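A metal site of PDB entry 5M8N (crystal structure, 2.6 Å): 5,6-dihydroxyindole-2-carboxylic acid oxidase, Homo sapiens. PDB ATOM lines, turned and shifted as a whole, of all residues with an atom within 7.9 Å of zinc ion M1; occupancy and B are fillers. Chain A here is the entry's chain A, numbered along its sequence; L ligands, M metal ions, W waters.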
ATOM      1  N   HIS A 168      18.201   4.060 -10.143  1.00  0.00           N
ATOM      2  CA  HIS A 168      19.017   3.108  -9.409  1.00  0.00           C
ATOM      3  C   HIS A 168      20.291   2.778 -10.198  1.00  0.00           C
ATOM      4  O   HIS A 168      21.375   2.688  -9.610  1.00  0.00           O
ATOM      5  CB  HIS A 168      18.195   1.849  -9.134  1.00  0.00           C
ATOM      6  CG  HIS A 168      18.843   0.874  -8.212  1.00  0.00           C
ATOM      7  ND1 HIS A 168      19.518  -0.233  -8.678  1.00  0.00           N
ATOM      8  CD2 HIS A 168      18.910   0.825  -6.863  1.00  0.00           C
ATOM      9  CE1 HIS A 168      19.966  -0.932  -7.643  1.00  0.00           C
ATOM     10  NE2 HIS A 168      19.618  -0.301  -6.533  1.00  0.00           N
ATOM     11  N   SER A 190      24.431   4.735  -3.886  1.00  0.00           N
ATOM     12  CA  SER A 190      23.254   4.203  -3.203  1.00  0.00           C
ATOM     13  C   SER A 190      23.497   2.924  -2.400  1.00  0.00           C
ATOM     14  O   SER A 190      22.549   2.423  -1.765  1.00  0.00           O
ATOM     15  CB  SER A 190      22.128   3.964  -4.216  1.00  0.00           C
ATOM     16  OG  SER A 190      22.642   3.437  -5.425  1.00  0.00           O
ATOM     17  N   HIS A 191      24.717   2.392  -2.418  1.00  0.00           N
ATOM     18  CA  HIS A 191      25.061   1.189  -1.670  1.00  0.00           C
ATOM     19  C   HIS A 191      26.418   1.377  -1.019  1.00  0.00           C
ATOM     20  O   HIS A 191      27.133   2.335  -1.297  1.00  0.00           O
ATOM     21  CB  HIS A 191      25.083  -0.048  -2.588  1.00  0.00           C
ATOM     22  CG  HIS A 191      23.856  -0.218  -3.396  1.00  0.00           C
ATOM     23  ND1 HIS A 191      23.686   0.386  -4.629  1.00  0.00           N
ATOM     24  CD2 HIS A 191      22.692  -0.862  -3.117  1.00  0.00           C
ATOM     25  CE1 HIS A 191      22.481   0.091  -5.090  1.00  0.00           C
ATOM     26  NE2 HIS A 191      21.858  -0.660  -4.197  1.00  0.00           N
ATOM     27  N   PHE A 196      22.677   4.231   1.830  1.00  0.00           N
ATOM     28  CA  PHE A 196      21.879   3.085   1.395  1.00  0.00           C
ATOM     29  C   PHE A 196      20.402   3.146   1.824  1.00  0.00           C
ATOM     30  O   PHE A 196      19.492   3.162   0.991  1.00  0.00           O
ATOM     31  CB  PHE A 196      22.562   1.809   1.913  1.00  0.00           C
ATOM     32  CG  PHE A 196      21.773   0.564   1.683  1.00  0.00           C
ATOM     33  CD1 PHE A 196      21.511   0.123   0.418  1.00  0.00           C
ATOM     34  CD2 PHE A 196      21.290  -0.180   2.753  1.00  0.00           C
ATOM     35  CE1 PHE A 196      20.772  -1.046   0.199  1.00  0.00           C
ATOM     36  CE2 PHE A 196      20.560  -1.336   2.563  1.00  0.00           C
ATOM     37  CZ  PHE A 196      20.297  -1.776   1.280  1.00  0.00           C
ATOM     38  N   HIS A 200      17.259   4.238  -0.710  1.00  0.00           N
ATOM     39  CA  HIS A 200      16.205   3.331  -1.140  1.00  0.00           C
ATOM     40  C   HIS A 200      14.855   3.732  -0.564  1.00  0.00           C
ATOM     41  O   HIS A 200      13.834   3.475  -1.207  1.00  0.00           O
ATOM     42  CB  HIS A 200      16.583   1.903  -0.771  1.00  0.00           C
ATOM     43  CG  HIS A 200      17.716   1.378  -1.605  1.00  0.00           C
ATOM     44  ND1 HIS A 200      19.021   1.821  -1.464  1.00  0.00           N
ATOM     45  CD2 HIS A 200      17.733   0.507  -2.651  1.00  0.00           C
ATOM     46  CE1 HIS A 200      19.794   1.214  -2.343  1.00  0.00           C
ATOM     47  NE2 HIS A 200      19.033   0.416  -3.081  1.00  0.00           N
ATOM     48  N   GLU A 336      21.931  -3.983   5.232  1.00  0.00           N
ATOM     49  CA  GLU A 336      22.371  -4.063   3.839  1.00  0.00           C
ATOM     50  C   GLU A 336      22.919  -5.435   3.511  1.00  0.00           C
ATOM     51  O   GLU A 336      22.604  -6.010   2.464  1.00  0.00           O
ATOM     52  CB  GLU A 336      23.414  -2.994   3.505  1.00  0.00           C
ATOM     53  CG  GLU A 336      23.878  -3.013   2.054  1.00  0.00           C
ATOM     54  CD  GLU A 336      24.606  -1.714   1.618  1.00  0.00           C
ATOM     55  OE1 GLU A 336      24.858  -0.841   2.486  1.00  0.00           O
ATOM     56  OE2 GLU A 336      24.964  -1.560   0.416  1.00  0.00           O
ATOM     57  N   HIS A 353      19.576  -7.980   3.377  1.00  0.00           N
ATOM     58  CA  HIS A 353      19.172  -7.354   2.112  1.00  0.00           C
ATOM     59  C   HIS A 353      19.957  -7.884   0.905  1.00  0.00           C
ATOM     60  O   HIS A 353      19.385  -8.062  -0.178  1.00  0.00           O
ATOM     61  CB  HIS A 353      19.324  -5.843   2.178  1.00  0.00           C
ATOM     62  CG  HIS A 353      19.501  -5.195   0.840  1.00  0.00           C
ATOM     63  ND1 HIS A 353      20.749  -4.876   0.326  1.00  0.00           N
ATOM     64  CD2 HIS A 353      18.601  -4.770  -0.079  1.00  0.00           C
ATOM     65  CE1 HIS A 353      20.608  -4.286  -0.839  1.00  0.00           C
ATOM     66  NE2 HIS A 353      19.313  -4.212  -1.115  1.00  0.00           N
ATOM     67  N   ASN A 354      21.275  -8.094   1.060  1.00  0.00           N
ATOM     68  CA  ASN A 354      22.086  -8.546  -0.071  1.00  0.00           C
ATOM     69  C   ASN A 354      21.848 -10.022  -0.369  1.00  0.00           C
ATOM     70  O   ASN A 354      21.855 -10.420  -1.533  1.00  0.00           O
ATOM     71  CB  ASN A 354      23.576  -8.310   0.174  1.00  0.00           C
ATOM     72  CG  ASN A 354      23.997  -6.863  -0.043  1.00  0.00           C
ATOM     73  OD1 ASN A 354      23.362  -6.093  -0.787  1.00  0.00           O
ATOM     74  ND2 ASN A 354      25.096  -6.472   0.605  1.00  0.00           N
ATOM     75  N   ALA A 356      18.969 -11.645   0.188  1.00  0.00           N
ATOM     76  CA  ALA A 356      17.712 -11.686  -0.557  1.00  0.00           C
ATOM     77  C   ALA A 356      17.951 -11.426  -2.038  1.00  0.00           C
ATOM     78  O   ALA A 356      17.332 -12.063  -2.896  1.00  0.00           O
ATOM     79  CB  ALA A 356      16.733 -10.660   0.000  1.00  0.00           C
ATOM     80  N   HIS A 357      18.842 -10.485  -2.373  1.00  0.00           N
ATOM     81  CA  HIS A 357      19.069 -10.144  -3.776  1.00  0.00           C
ATOM     82  C   HIS A 357      19.681 -11.311  -4.524  1.00  0.00           C
ATOM     83  O   HIS A 357      19.198 -11.723  -5.579  1.00  0.00           O
ATOM     84  CB  HIS A 357      19.976  -8.911  -3.901  1.00  0.00           C
ATOM     85  CG  HIS A 357      19.223  -7.613  -4.003  1.00  0.00           C
ATOM     86  ND1 HIS A 357      18.450  -7.290  -5.100  1.00  0.00           N
ATOM     87  CD2 HIS A 357      19.133  -6.564  -3.150  1.00  0.00           C
ATOM     88  CE1 HIS A 357      17.912  -6.096  -4.916  1.00  0.00           C
ATOM     89  NE2 HIS A 357      18.307  -5.639  -3.739  1.00  0.00           N
ATOM     90  N   GLY A 364      17.545  -9.772 -10.562  1.00  0.00           N
ATOM     91  CA  GLY A 364      17.434  -9.089  -9.291  1.00  0.00           C
ATOM     92  C   GLY A 364      18.656  -9.176  -8.432  1.00  0.00           C
ATOM     93  O   GLY A 364      18.717  -8.526  -7.386  1.00  0.00           O
ATOM     94  N   THR A 367      23.431  -5.380  -9.373  1.00  0.00           N
ATOM     95  CA  THR A 367      23.130  -4.076  -8.859  1.00  0.00           C
ATOM     96  C   THR A 367      22.668  -3.074  -9.866  1.00  0.00           C
ATOM     97  O   THR A 367      21.758  -2.344  -9.606  1.00  0.00           O
ATOM     98  CB  THR A 367      24.314  -3.517  -8.094  1.00  0.00           C
ATOM     99  OG1 THR A 367      24.867  -4.573  -7.337  1.00  0.00           O
ATOM    100  CG2 THR A 367      23.899  -2.424  -7.175  1.00  0.00           C
ATOM    101  N   SER A 370      18.912  -4.680 -10.890  1.00  0.00           N
ATOM    102  CA  SER A 370      17.972  -5.402 -10.037  1.00  0.00           C
ATOM    103  C   SER A 370      16.556  -4.825  -9.984  1.00  0.00           C
ATOM    104  O   SER A 370      15.627  -5.634  -9.839  1.00  0.00           O
ATOM    105  CB  SER A 370      18.555  -5.540  -8.634  1.00  0.00           C
ATOM    106  OG  SER A 370      18.804  -4.264  -8.094  1.00  0.00           O
ATOM    107  N   PRO A 371      16.301  -3.517 -10.056  1.00  0.00           N
ATOM    108  CA  PRO A 371      14.888  -3.067 -10.019  1.00  0.00           C
ATOM    109  C   PRO A 371      14.088  -3.539 -11.208  1.00  0.00           C
ATOM    110  O   PRO A 371      12.859  -3.398 -11.196  1.00  0.00           O
ATOM    111  CB  PRO A 371      15.003  -1.530  -9.978  1.00  0.00           C
ATOM    112  CG  PRO A 371      16.348  -1.282  -9.447  1.00  0.00           C
ATOM    113  CD  PRO A 371      17.207  -2.352 -10.079  1.00  0.00           C
ATOM    114  N   PHE A 376      12.052  -6.452  -6.406  1.00  0.00           N
ATOM    115  CA  PHE A 376      12.873  -5.380  -5.842  1.00  0.00           C
ATOM    116  C   PHE A 376      12.068  -4.471  -4.940  1.00  0.00           C
ATOM    117  O   PHE A 376      12.453  -4.199  -3.803  1.00  0.00           O
ATOM    118  CB  PHE A 376      13.497  -4.570  -6.982  1.00  0.00           C
ATOM    119  CG  PHE A 376      14.465  -3.552  -6.515  1.00  0.00           C
ATOM    120  CD1 PHE A 376      14.036  -2.260  -6.196  1.00  0.00           C
ATOM    121  CD2 PHE A 376      15.811  -3.864  -6.405  1.00  0.00           C
ATOM    122  CE1 PHE A 376      14.935  -1.318  -5.762  1.00  0.00           C
ATOM    123  CE2 PHE A 376      16.715  -2.928  -5.983  1.00  0.00           C
ATOM    124  CZ  PHE A 376      16.271  -1.653  -5.652  1.00  0.00           C
ATOM    125  N   LEU A 379      11.235  -6.432  -1.949  1.00  0.00           N
ATOM    126  CA  LEU A 379      12.483  -6.648  -1.206  1.00  0.00           C
ATOM    127  C   LEU A 379      12.883  -5.380  -0.479  1.00  0.00           C
ATOM    128  O   LEU A 379      13.332  -5.415   0.674  1.00  0.00           O
ATOM    129  CB  LEU A 379      13.572  -7.117  -2.169  1.00  0.00           C
ATOM    130  CG  LEU A 379      14.922  -7.698  -1.692  1.00  0.00           C
ATOM    131  CD1 LEU A 379      15.739  -8.090  -2.902  1.00  0.00           C
ATOM    132  CD2 LEU A 379      15.766  -6.786  -0.752  1.00  0.00           C
ATOM    133  N   HIS A 380      12.655  -4.235  -1.091  1.00  0.00           N
ATOM    134  CA  HIS A 380      13.109  -2.999  -0.477  1.00  0.00           C
ATOM    135  C   HIS A 380      12.098  -2.337   0.434  1.00  0.00           C
ATOM    136  O   HIS A 380      12.526  -1.576   1.312  1.00  0.00           O
ATOM    137  CB  HIS A 380      13.570  -2.030  -1.556  1.00  0.00           C
ATOM    138  CG  HIS A 380      15.000  -2.226  -1.888  1.00  0.00           C
ATOM    139  ND1 HIS A 380      16.006  -1.793  -1.059  1.00  0.00           N
ATOM    140  CD2 HIS A 380      15.601  -2.938  -2.870  1.00  0.00           C
ATOM    141  CE1 HIS A 380      17.166  -2.179  -1.548  1.00  0.00           C
ATOM    142  NE2 HIS A 380      16.949  -2.870  -2.651  1.00  0.00           N
ATOM    143  N   THR A 383      12.896  -3.875   3.553  1.00  0.00           N
ATOM    144  CA  THR A 383      14.136  -3.273   4.072  1.00  0.00           C
ATOM    145  C   THR A 383      13.852  -1.938   4.725  1.00  0.00           C
ATOM    146  O   THR A 383      14.373  -1.651   5.809  1.00  0.00           O
ATOM    147  CB  THR A 383      15.154  -3.102   2.925  1.00  0.00           C
ATOM    148  OG1 THR A 383      15.422  -4.377   2.309  1.00  0.00           O
ATOM    149  CG2 THR A 383      16.481  -2.527   3.421  1.00  0.00           C
HETATM  150  O1  LIG L   1      21.872  -3.820  -4.017  1.00  0.00           O
HETATM  151  C1  LIG L   1      26.756  -8.098  -3.249  1.00  0.00           C
HETATM  152  O2  LIG L   1      26.361  -8.827  -2.357  1.00  0.00           O
HETATM  153  O3  LIG L   1      27.951  -8.087  -3.601  1.00  0.00           O
HETATM  154  N1  LIG L   1      26.321  -7.063  -5.281  1.00  0.00           N
HETATM  155  C2  LIG L   1      25.774  -7.204  -3.958  1.00  0.00           C
HETATM  156  C3  LIG L   1      24.395  -7.852  -3.932  1.00  0.00           C
HETATM  157  N2  LIG L   1      23.446  -7.014  -4.593  1.00  0.00           N
HETATM  158  C4  LIG L   1      23.057  -5.765  -3.971  1.00  0.00           C
HETATM  159  C5  LIG L   1      22.847  -7.372  -5.882  1.00  0.00           C
HETATM  160  C6  LIG L   1      22.204  -4.999  -4.569  1.00  0.00           C
HETATM  161  C7  LIG L   1      21.977  -6.593  -6.468  1.00  0.00           C
HETATM  162  C8  LIG L   1      21.597  -5.321  -5.863  1.00  0.00           C
HETATM  163  O4  LIG L   1      20.843  -4.578  -6.358  1.00  0.00           O
HETATM  164 ZN    ZN M   1      18.728  -3.738  -2.953  1.00  0.00          ZN
HETATM  165 ZN    ZN M   2      19.853  -0.718  -4.610  1.00  0.00          ZN
HETATM  166  O   HOH W   1      19.732  -2.796  -4.435  1.00  0.00           O
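NE2 of His 191 lies close to O1 of the ligand (3.2 Å). The side-chain hydroxyl of Ser 370 lies within hydrogen-bond range of an oxygen (O4) of the ligand (2.7 Å).
Zinc ion M1 is bound by a ring nitrogen (NE2) of His 353, a ring nitrogen (NE2) of His 380, water W1 and a ring nitrogen (NE2) of His 357. Zinc ion M1 has four donor atoms within binding distance.
Phe 376 touches zinc ion M1. Within 4 Å of zinc ion M1: His 353, His 357, Phe 376 and His 380.
A ring nitrogen (ND1) of His 353 lies within hydrogen-bond range of the side-chain amide oxygen (OD1) of Asn 354. ND1 of His 353 is in hydrogen-bond range of O of Glu 336. O of Gly 364 lies within hydrogen-bond range of ND1 of His 357 (2.6 Å).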
